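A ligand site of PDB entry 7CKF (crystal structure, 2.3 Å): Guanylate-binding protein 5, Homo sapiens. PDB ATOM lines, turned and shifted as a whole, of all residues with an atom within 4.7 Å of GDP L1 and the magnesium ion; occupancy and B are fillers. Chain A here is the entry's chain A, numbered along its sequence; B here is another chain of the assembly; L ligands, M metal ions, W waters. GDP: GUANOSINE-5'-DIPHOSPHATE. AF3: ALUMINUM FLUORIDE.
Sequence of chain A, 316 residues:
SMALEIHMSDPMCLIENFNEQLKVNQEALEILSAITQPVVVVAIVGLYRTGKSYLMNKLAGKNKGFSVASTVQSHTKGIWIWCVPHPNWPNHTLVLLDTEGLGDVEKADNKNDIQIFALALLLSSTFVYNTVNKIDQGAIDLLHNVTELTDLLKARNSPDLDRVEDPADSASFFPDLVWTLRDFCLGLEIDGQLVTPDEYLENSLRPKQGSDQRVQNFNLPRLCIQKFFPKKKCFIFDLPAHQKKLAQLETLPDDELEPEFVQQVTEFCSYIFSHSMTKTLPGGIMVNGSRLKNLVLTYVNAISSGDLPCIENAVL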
ATOM      1  N   LEU A  47      22.040 -20.640  11.811  1.00  0.00           N
ATOM      2  CA  LEU A  47      22.851 -20.111  12.902  1.00  0.00           C
ATOM      3  C   LEU A  47      22.228 -18.812  13.415  1.00  0.00           C
ATOM      4  O   LEU A  47      21.500 -18.130  12.712  1.00  0.00           O
ATOM      5  CB  LEU A  47      24.294 -19.867  12.469  1.00  0.00           C
ATOM      6  CG  LEU A  47      25.095 -21.037  11.869  1.00  0.00           C
ATOM      7  CD1 LEU A  47      26.533 -20.599  11.632  1.00  0.00           C
ATOM      8  CD2 LEU A  47      25.064 -22.286  12.759  1.00  0.00           C
ATOM      9  N   TYR A  48      22.514 -18.470  14.663  1.00  0.00           N
ATOM     10  CA  TYR A  48      21.881 -17.280  15.210  1.00  0.00           C
ATOM     11  C   TYR A  48      22.374 -16.017  14.489  1.00  0.00           C
ATOM     12  O   TYR A  48      23.403 -16.024  13.790  1.00  0.00           O
ATOM     13  CB  TYR A  48      22.093 -17.182  16.729  1.00  0.00           C
ATOM     14  CG  TYR A  48      23.461 -16.747  17.211  1.00  0.00           C
ATOM     15  CD1 TYR A  48      24.632 -17.328  16.691  1.00  0.00           C
ATOM     16  CD2 TYR A  48      23.583 -15.810  18.231  1.00  0.00           C
ATOM     17  CE1 TYR A  48      25.865 -16.952  17.141  1.00  0.00           C
ATOM     18  CE2 TYR A  48      24.841 -15.433  18.708  1.00  0.00           C
ATOM     19  CZ  TYR A  48      25.966 -16.012  18.166  1.00  0.00           C
ATOM     20  OH  TYR A  48      27.207 -15.642  18.617  1.00  0.00           O
ATOM     21  N   ARG A  49      21.560 -14.938  14.592  1.00  0.00           N
ATOM     22  CA  ARG A  49      21.880 -13.595  14.084  1.00  0.00           C
ATOM     23  C   ARG A  49      21.929 -13.583  12.566  1.00  0.00           C
ATOM     24  O   ARG A  49      22.728 -12.861  11.966  1.00  0.00           O
ATOM     25  CB  ARG A  49      23.196 -13.056  14.648  1.00  0.00           C
ATOM     26  CG  ARG A  49      23.337 -13.215  16.130  1.00  0.00           C
ATOM     27  CD  ARG A  49      22.632 -12.137  16.883  1.00  0.00           C
ATOM     28  NE  ARG A  49      21.187 -12.362  16.867  1.00  0.00           N
ATOM     29  CZ  ARG A  49      20.289 -11.413  16.667  1.00  0.00           C
ATOM     30  NH1 ARG A  49      20.692 -10.162  16.479  1.00  0.00           N
ATOM     31  NH2 ARG A  49      18.988 -11.710  16.640  1.00  0.00           N
ATOM     32  N   THR A  50      21.047 -14.354  11.953  1.00  0.00           N
ATOM     33  CA  THR A  50      21.110 -14.616  10.531  1.00  0.00           C
ATOM     34  C   THR A  50      19.843 -14.141   9.824  1.00  0.00           C
ATOM     35  O   THR A  50      19.621 -14.439   8.639  1.00  0.00           O
ATOM     36  CB  THR A  50      21.423 -16.120  10.404  1.00  0.00           C
ATOM     37  OG1 THR A  50      22.519 -16.335   9.507  1.00  0.00           O
ATOM     38  CG2 THR A  50      20.250 -16.992  10.108  1.00  0.00           C
ATOM     39  N   GLY A  51      19.025 -13.347  10.521  1.00  0.00           N
ATOM     40  CA  GLY A  51      17.838 -12.766   9.921  1.00  0.00           C
ATOM     41  C   GLY A  51      16.732 -13.756   9.697  1.00  0.00           C
ATOM     42  O   GLY A  51      15.945 -13.567   8.767  1.00  0.00           O
ATOM     43  N   LYS A  52      16.664 -14.822  10.497  1.00  0.00           N
ATOM     44  CA  LYS A  52      15.598 -15.805  10.338  1.00  0.00           C
ATOM     45  C   LYS A  52      14.246 -15.173  10.648  1.00  0.00           C
ATOM     46  O   LYS A  52      13.339 -15.170   9.814  1.00  0.00           O
ATOM     47  CB  LYS A  52      15.831 -17.015  11.251  1.00  0.00           C
ATOM     48  CG  LYS A  52      17.081 -17.824  10.910  1.00  0.00           C
ATOM     49  CD  LYS A  52      17.282 -19.029  11.820  1.00  0.00           C
ATOM     50  CE  LYS A  52      17.493 -18.564  13.252  1.00  0.00           C
ATOM     51  NZ  LYS A  52      18.689 -17.672  13.322  1.00  0.00           N
ATOM     52  N   SER A  53      14.136 -14.614  11.859  1.00  0.00           N
ATOM     53  CA  SER A  53      12.902 -13.982  12.316  1.00  0.00           C
ATOM     54  C   SER A  53      12.398 -12.934  11.337  1.00  0.00           C
ATOM     55  O   SER A  53      11.193 -12.825  11.092  1.00  0.00           O
ATOM     56  CB  SER A  53      13.138 -13.388  13.700  1.00  0.00           C
ATOM     57  OG  SER A  53      12.952 -14.362  14.702  1.00  0.00           O
ATOM     58  N   TYR A  54      13.306 -12.135  10.791  1.00  0.00           N
ATOM     59  CA  TYR A  54      12.909 -11.123   9.819  1.00  0.00           C
ATOM     60  C   TYR A  54      12.282 -11.772   8.588  1.00  0.00           C
ATOM     61  O   TYR A  54      11.240 -11.318   8.098  1.00  0.00           O
ATOM     62  CB  TYR A  54      14.127 -10.270   9.437  1.00  0.00           C
ATOM     63  CG  TYR A  54      13.833  -9.247   8.380  1.00  0.00           C
ATOM     64  CD1 TYR A  54      13.244  -8.023   8.699  1.00  0.00           C
ATOM     65  CD2 TYR A  54      14.145  -9.492   7.054  1.00  0.00           C
ATOM     66  CE1 TYR A  54      12.960  -7.075   7.721  1.00  0.00           C
ATOM     67  CE2 TYR A  54      13.889  -8.557   6.063  1.00  0.00           C
ATOM     68  CZ  TYR A  54      13.289  -7.351   6.406  1.00  0.00           C
ATOM     69  OH  TYR A  54      13.042  -6.438   5.410  1.00  0.00           O
ATOM     70  N   SER A  67       9.806 -11.155  16.725  1.00  0.00           N
ATOM     71  CA  SER A  67      10.659 -10.042  17.110  1.00  0.00           C
ATOM     72  C   SER A  67      12.057 -10.234  16.545  1.00  0.00           C
ATOM     73  O   SER A  67      12.572 -11.353  16.524  1.00  0.00           O
ATOM     74  CB  SER A  67      10.706  -9.960  18.632  1.00  0.00           C
ATOM     75  OG  SER A  67      11.373  -8.803  19.066  1.00  0.00           O
ATOM     76  N   VAL A  68      12.696  -9.153  16.075  1.00  0.00           N
ATOM     77  CA  VAL A  68      14.011  -9.325  15.482  1.00  0.00           C
ATOM     78  C   VAL A  68      15.171  -8.901  16.408  1.00  0.00           C
ATOM     79  O   VAL A  68      15.900  -9.783  16.885  1.00  0.00           O
ATOM     80  CB  VAL A  68      14.088  -8.665  14.089  1.00  0.00           C
ATOM     81  CG1 VAL A  68      13.054  -9.318  13.188  1.00  0.00           C
ATOM     82  CG2 VAL A  68      13.810  -7.200  14.131  1.00  0.00           C
ATOM     83  N   ALA A  69      15.392  -7.605  16.651  1.00  0.00           N
ATOM     84  CA  ALA A  69      16.584  -7.166  17.431  1.00  0.00           C
ATOM     85  C   ALA A  69      17.932  -7.305  16.718  1.00  0.00           C
ATOM     86  O   ALA A  69      18.140  -8.213  15.926  1.00  0.00           O
ATOM     87  CB  ALA A  69      16.698  -7.900  18.776  1.00  0.00           C
ATOM     88  N   SER A  70      18.896  -6.426  17.089  1.00  0.00           N
ATOM     89  CA  SER A  70      20.048  -6.150  16.235  1.00  0.00           C
ATOM     90  C   SER A  70      21.417  -6.137  16.924  1.00  0.00           C
ATOM     91  O   SER A  70      22.364  -5.555  16.380  1.00  0.00           O
ATOM     92  CB  SER A  70      19.831  -4.807  15.529  1.00  0.00           C
ATOM     93  OG  SER A  70      18.621  -4.832  14.771  1.00  0.00           O
ATOM     94  N   THR A  76      15.693 -14.536  19.646  1.00  0.00           N
ATOM     95  CA  THR A  76      14.685 -15.578  19.694  1.00  0.00           C
ATOM     96  C   THR A  76      15.128 -16.739  20.574  1.00  0.00           C
ATOM     97  O   THR A  76      16.253 -17.245  20.414  1.00  0.00           O
ATOM     98  CB  THR A  76      14.390 -16.099  18.281  1.00  0.00           C
ATOM     99  OG1 THR A  76      14.128 -15.008  17.389  1.00  0.00           O
ATOM    100  CG2 THR A  76      13.202 -17.070  18.283  1.00  0.00           C
ATOM    101  N   ASP A  98       9.297 -20.243  13.990  1.00  0.00           N
ATOM    102  CA  ASP A  98      10.500 -19.434  14.086  1.00  0.00           C
ATOM    103  C   ASP A  98      11.310 -19.937  15.279  1.00  0.00           C
ATOM    104  O   ASP A  98      10.771 -20.060  16.382  1.00  0.00           O
ATOM    105  CB  ASP A  98      10.113 -17.972  14.281  1.00  0.00           C
ATOM    106  CG  ASP A  98      11.294 -17.049  14.224  1.00  0.00           C
ATOM    107  OD1 ASP A  98      12.260 -17.392  13.479  1.00  0.00           O
ATOM    108  OD2 ASP A  98      11.246 -15.987  14.889  1.00  0.00           O
ATOM    109  N   THR A  99      12.588 -20.226  15.056  1.00  0.00           N
ATOM    110  CA  THR A  99      13.372 -20.970  16.039  1.00  0.00           C
ATOM    111  C   THR A  99      14.574 -20.185  16.553  1.00  0.00           C
ATOM    112  O   THR A  99      15.124 -19.313  15.879  1.00  0.00           O
ATOM    113  CB  THR A  99      13.868 -22.300  15.442  1.00  0.00           C
ATOM    114  OG1 THR A  99      14.900 -22.042  14.473  1.00  0.00           O
ATOM    115  CG2 THR A  99      12.714 -23.028  14.757  1.00  0.00           C
ATOM    116  N   ARG A 182      21.596 -15.952   2.391  1.00  0.00           N
ATOM    117  CA  ARG A 182      21.479 -14.534   2.694  1.00  0.00           C
ATOM    118  C   ARG A 182      22.783 -13.806   2.392  1.00  0.00           C
ATOM    119  O   ARG A 182      23.862 -14.402   2.396  1.00  0.00           O
ATOM    120  CB  ARG A 182      21.084 -14.325   4.169  1.00  0.00           C
ATOM    121  CG  ARG A 182      19.949 -15.234   4.644  1.00  0.00           C
ATOM    122  CD  ARG A 182      18.607 -14.856   4.067  1.00  0.00           C
ATOM    123  NE  ARG A 182      18.118 -13.591   4.635  1.00  0.00           N
ATOM    124  CZ  ARG A 182      17.378 -13.488   5.739  1.00  0.00           C
ATOM    125  NH1 ARG A 182      17.019 -14.563   6.417  1.00  0.00           N
ATOM    126  NH2 ARG A 182      17.013 -12.288   6.171  1.00  0.00           N
ATOM    127  N   ASP A 183      22.660 -12.503   2.129  1.00  0.00           N
ATOM    128  CA  ASP A 183      23.797 -11.628   1.843  1.00  0.00           C
ATOM    129  C   ASP A 183      24.722 -12.273   0.807  1.00  0.00           C
ATOM    130  O   ASP A 183      25.917 -12.489   1.027  1.00  0.00           O
ATOM    131  CB  ASP A 183      24.554 -11.277   3.143  1.00  0.00           C
ATOM    132  CG  ASP A 183      23.643 -10.592   4.190  1.00  0.00           C
ATOM    133  OD1 ASP A 183      22.515 -10.087   3.853  1.00  0.00           O
ATOM    134  OD2 ASP A 183      24.069 -10.512   5.370  1.00  0.00           O
ATOM    135  N   ASP A 238      19.963 -10.813  -1.870  1.00  0.00           N
ATOM    136  CA  ASP A 238      20.974  -9.785  -1.737  1.00  0.00           C
ATOM    137  C   ASP A 238      21.042  -9.302  -0.292  1.00  0.00           C
ATOM    138  O   ASP A 238      20.187  -9.616   0.543  1.00  0.00           O
ATOM    139  CB  ASP A 238      20.656  -8.578  -2.634  1.00  0.00           C
ATOM    140  CG  ASP A 238      20.860  -8.898  -4.108  1.00  0.00           C
ATOM    141  OD1 ASP A 238      21.121 -10.075  -4.426  1.00  0.00           O
ATOM    142  OD2 ASP A 238      20.745  -7.967  -4.935  1.00  0.00           O
ATOM    143  N   LEU A 239      22.097  -8.540   0.015  1.00  0.00           N
ATOM    144  CA  LEU A 239      22.047  -7.666   1.179  1.00  0.00           C
ATOM    145  C   LEU A 239      20.836  -6.758   1.065  1.00  0.00           C
ATOM    146  O   LEU A 239      20.670  -6.088   0.035  1.00  0.00           O
ATOM    147  CB  LEU A 239      23.327  -6.831   1.284  1.00  0.00           C
ATOM    148  CG  LEU A 239      24.532  -7.585   1.870  1.00  0.00           C
ATOM    149  CD1 LEU A 239      25.841  -7.179   1.191  1.00  0.00           C
ATOM    150  CD2 LEU A 239      24.598  -7.383   3.385  1.00  0.00           C
ATOM    151  N   PRO A 240      19.966  -6.764   2.032  1.00  0.00           N
ATOM    152  CA  PRO A 240      18.759  -5.978   1.964  1.00  0.00           C
ATOM    153  C   PRO A 240      18.897  -4.477   1.948  1.00  0.00           C
ATOM    154  O   PRO A 240      18.167  -3.852   1.261  1.00  0.00           O
ATOM    155  CB  PRO A 240      18.000  -6.403   3.183  1.00  0.00           C
ATOM    156  CG  PRO A 240      18.971  -7.025   4.057  1.00  0.00           C
ATOM    157  CD  PRO A 240      20.030  -7.574   3.221  1.00  0.00           C
ATOM    158  N   LEU A 246      21.153  -1.932   8.600  1.00  0.00           N
ATOM    159  CA  LEU A 246      20.534  -3.130   8.901  1.00  0.00           C
ATOM    160  C   LEU A 246      19.890  -3.139  10.249  1.00  0.00           C
ATOM    161  O   LEU A 246      19.005  -3.863  10.391  1.00  0.00           O
ATOM    162  CB  LEU A 246      21.573  -4.210   8.749  1.00  0.00           C
ATOM    163  CG  LEU A 246      22.043  -4.304   7.310  1.00  0.00           C
ATOM    164  CD1 LEU A 246      23.348  -5.029   7.142  1.00  0.00           C
ATOM    165  CD2 LEU A 246      20.988  -4.880   6.402  1.00  0.00           C
ATOM    166  N   ALA A 247      20.310  -2.349  11.233  1.00  0.00           N
ATOM    167  CA  ALA A 247      19.646  -2.553  12.521  1.00  0.00           C
ATOM    168  C   ALA A 247      18.202  -2.043  12.550  1.00  0.00           C
ATOM    169  O   ALA A 247      17.439  -2.418  13.443  1.00  0.00           O
ATOM    170  CB  ALA A 247      20.460  -1.854  13.621  1.00  0.00           C
ATOM    171  N   LEU A 249      16.097  -2.445   9.934  1.00  0.00           N
ATOM    172  CA  LEU A 249      15.510  -3.032   8.730  1.00  0.00           C
ATOM    173  C   LEU A 249      14.003  -3.227   8.858  1.00  0.00           C
ATOM    174  O   LEU A 249      13.260  -2.989   7.902  1.00  0.00           O
ATOM    175  CB  LEU A 249      16.195  -4.365   8.422  1.00  0.00           C
ATOM    176  CG  LEU A 249      16.155  -4.840   6.975  1.00  0.00           C
ATOM    177  CD1 LEU A 249      16.923  -3.889   6.063  1.00  0.00           C
ATOM    178  CD2 LEU A 249      16.748  -6.243   6.917  1.00  0.00           C
ATOM    179  N   PHE A 261      16.436  -7.325  -3.666  1.00  0.00           N
ATOM    180  CA  PHE A 261      16.061  -8.041  -2.451  1.00  0.00           C
ATOM    181  C   PHE A 261      14.549  -8.151  -2.305  1.00  0.00           C
ATOM    182  O   PHE A 261      14.026  -9.200  -1.899  1.00  0.00           O
ATOM    183  CB  PHE A 261      16.655  -7.350  -1.230  1.00  0.00           C
ATOM    184  CG  PHE A 261      16.221  -7.974   0.063  1.00  0.00           C
ATOM    185  CD1 PHE A 261      16.847  -9.126   0.531  1.00  0.00           C
ATOM    186  CD2 PHE A 261      15.148  -7.446   0.797  1.00  0.00           C
ATOM    187  CE1 PHE A 261      16.436  -9.732   1.715  1.00  0.00           C
ATOM    188  CE2 PHE A 261      14.742  -8.044   1.976  1.00  0.00           C
ATOM    189  CZ  PHE A 261      15.383  -9.191   2.426  1.00  0.00           C
ATOM    190  N   LEU B 186      26.523  -5.941  13.445  1.00  0.00           N
ATOM    191  CA  LEU B 186      25.691  -6.092  14.634  1.00  0.00           C
ATOM    192  C   LEU B 186      26.121  -5.103  15.714  1.00  0.00           C
ATOM    193  O   LEU B 186      27.259  -4.633  15.720  1.00  0.00           O
ATOM    194  CB  LEU B 186      25.771  -7.534  15.131  1.00  0.00           C
ATOM    195  CG  LEU B 186      25.077  -8.527  14.195  1.00  0.00           C
ATOM    196  CD1 LEU B 186      25.418  -9.953  14.543  1.00  0.00           C
ATOM    197  CD2 LEU B 186      23.577  -8.325  14.266  1.00  0.00           C
HETATM  198  PB  GDP L   1      17.723 -14.163  13.799  1.00  0.00           P
HETATM  199  O1B GDP L   1      18.485 -14.318  15.091  1.00  0.00           O
HETATM  200  O2B GDP L   1      16.260 -14.418  14.059  1.00  0.00           O
HETATM  201  O3B GDP L   1      18.224 -15.113  12.725  1.00  0.00           O
HETATM  202  O3A GDP L   1      17.976 -12.700  13.184  1.00  0.00           O
HETATM  203  PA  GDP L   1      16.855 -11.544  13.232  1.00  0.00           P
HETATM  204  O1A GDP L   1      16.407 -11.325  14.672  1.00  0.00           O
HETATM  205  O2A GDP L   1      15.703 -11.901  12.329  1.00  0.00           O
HETATM  206  O5' GDP L   1      17.696 -10.352  12.574  1.00  0.00           O
HETATM  207  C5' GDP L   1      18.990 -10.066  13.072  1.00  0.00           C
HETATM  208  C4' GDP L   1      19.494  -8.733  12.521  1.00  0.00           C
HETATM  209  O4' GDP L   1      19.791  -8.855  11.140  1.00  0.00           O
HETATM  210  C3' GDP L   1      18.454  -7.617  12.586  1.00  0.00           C
HETATM  211  O3' GDP L   1      19.203  -6.423  12.814  1.00  0.00           O
HETATM  212  C2' GDP L   1      17.901  -7.505  11.190  1.00  0.00           C
HETATM  213  O2' GDP L   1      17.435  -6.181  10.898  1.00  0.00           O
HETATM  214  C1' GDP L   1      19.129  -7.848  10.371  1.00  0.00           C
HETATM  215  N9  GDP L   1      18.813  -8.513   9.107  1.00  0.00           N
HETATM  216  C8  GDP L   1      17.644  -9.066   8.758  1.00  0.00           C
HETATM  217  N7  GDP L   1      17.743  -9.660   7.545  1.00  0.00           N
HETATM  218  C5  GDP L   1      19.009  -9.505   7.119  1.00  0.00           C
HETATM  219  C6  GDP L   1      19.790  -9.893   5.922  1.00  0.00           C
HETATM  220  O6  GDP L   1      19.231 -10.530   4.988  1.00  0.00           O
HETATM  221  N1  GDP L   1      21.092  -9.538   5.873  1.00  0.00           N
HETATM  222  C2  GDP L   1      21.689  -8.861   6.879  1.00  0.00           C
HETATM  223  N2  GDP L   1      23.011  -8.529   6.778  1.00  0.00           N
HETATM  224  N3  GDP L   1      21.026  -8.475   8.005  1.00  0.00           N
HETATM  225  C4  GDP L   1      19.719  -8.765   8.162  1.00  0.00           C
HETATM  226 AL   AF3 L   2      18.555 -15.932  16.813  1.00  0.00          AL
HETATM  227  F1  AF3 L   2      17.158 -15.311  16.690  1.00  0.00           F
HETATM  228  F2  AF3 L   2      18.861 -17.054  15.688  1.00  0.00           F
HETATM  229  F3  AF3 L   2      19.844 -15.029  17.242  1.00  0.00           F
HETATM  230 MG    MG M   1      15.106 -14.940  15.545  1.00  0.00          MG
HETATM  231  O   HOH W   1      25.752  -8.296   8.159  1.00  0.00           O
HETATM  232  O   HOH W   2      21.478 -11.468  10.142  1.00  0.00           O
HETATM  233  O   HOH W   3      21.617  -5.708  12.115  1.00  0.00           O
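Ala 69 touches GDP L1 (O to C3', 3.4 Å).
CD2 of Leu 239 touches N2 of GDP L1, 3.9 Å away.
CD of Pro 240 touches N1 of GDP L1, at 3.5 Å.
Ala 247 touches GDP L1.
CB of Leu 249 touches O2' of GDP L1, at 3.3 Å.
Hydrophobic or aromatic side chains within 4 Å of GDP L1: Tyr 54, Val 68, Leu 239, Pro 240, Leu 246 and Leu 249.
17 residues have an atom within 4 Å of GDP L1: Arg 49, Thr 50, Gly 51, Lys 52, Ser 53, Tyr 54, Val 68, Ala 69, Ser 70, Thr 76, Arg 182, Asp 183, Leu 239, Pro 240, Leu 246, Ala 247 and Leu 249.
An oxygen (O1B) of GDP L1 is bound to an aluminium atom (AL) of AF3 L2.
OG of Ser 53 lies close to OD1 of Asp 98, at 3.3 Å.
O of Ala 247 lies within hydrogen-bond range of OG of Ser 70 (3.0 Å).
O of Leu 47 lies within hydrogen-bond range of NZ of Lys 52, 2.9 Å away.
O of Gly 51 sits at hydrogen-bond distance from NH1 of Arg 182 (2.8 Å).
The guanidinium group of Arg 182 is in hydrogen-bond range of the backbone carbonyl oxygen of Thr 50 (3.4 Å).
The backbone carbonyl oxygen of Ala 69 is in hydrogen-bond range of the guanidinium group of Arg 49 (3.3 Å).
The magnesium ion is bound by O2B of GDP L1 (2.0 Å), OG1 of Thr 76 (2.1 Å), F1 of AF3 L2 (2.4 Å) and OG of Ser 53 (2.4 Å).
Along chain A the residues within 4 Å of the magnesium ion span positions 53 to 76.
The nearest printed residue that does not touch the magnesium ion is Asp 98 (4.1 Å).
The backbone NH (N) of Ser 53 is in hydrogen-bond range of an oxygen (O2A) of GDP L1 (3.2 Å).
The side-chain carboxylate of Asp 183 lies within hydrogen-bond range of a nitrogen (N1) of GDP L1.
An oxygen (O3') of GDP L1 is in hydrogen-bond range of the side-chain hydroxyl (OG) of Ser 70 (2.6 Å).
N of Lys 52 sits at hydrogen-bond distance from O3B of GDP L1.
The side-chain amino group (NZ) of Lys 52 lies within salt-bridge range of an oxygen (O3B) of GDP L1, 2.7 Å away.
An oxygen (O1A) of GDP L1 lies close to the backbone carbonyl oxygen of Val 68.
An oxygen (O2') of GDP L1 is in hydrogen-bond range of the backbone carbonyl oxygen of Leu 246.
O2A of GDP L1 sits at hydrogen-bond distance from N of Tyr 54, 2.9 Å away.
The backbone NH of Gly 51 lies within hydrogen-bond range of an oxygen (O3A) of GDP L1, 2.9 Å away.
The backbone NH (N) of Thr 50 is in hydrogen-bond range of an oxygen (O3B) of GDP L1, at 3.0 Å.
NH2 of Arg 182 is in hydrogen-bond range of N7 of GDP L1 (3.1 Å).
N of Arg 49 sits close to O1B of GDP L1 (3.2 Å).
The guanidinium group of Arg 49 is in salt-bridge range of an oxygen (O1A) of GDP L1 (3.3 Å).
The backbone NH (N) of Thr 76 lies close to a fluorine (F1) of AF3 L2 (3.4 Å).
A fluorine (F2) of AF3 L2 sits at hydrogen-bond distance from the side-chain amino group (NZ) of Lys 52 (2.5 Å).
A fluorine (F3) of AF3 L2 is in hydrogen-bond range of the backbone NH (N) of Arg 49 (3.2 Å).
The guanidinium group of Arg 49 lies within hydrogen-bond range of a fluorine (F3) of AF3 L2, 3.0 Å away.
Water W2 lies within hydrogen-bond range of O of Arg 49 (2.6 Å), N of Gly 51 (3.1 Å), O4' of GDP L1 (3.3 Å) and N of Thr 50 (3.4 Å).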
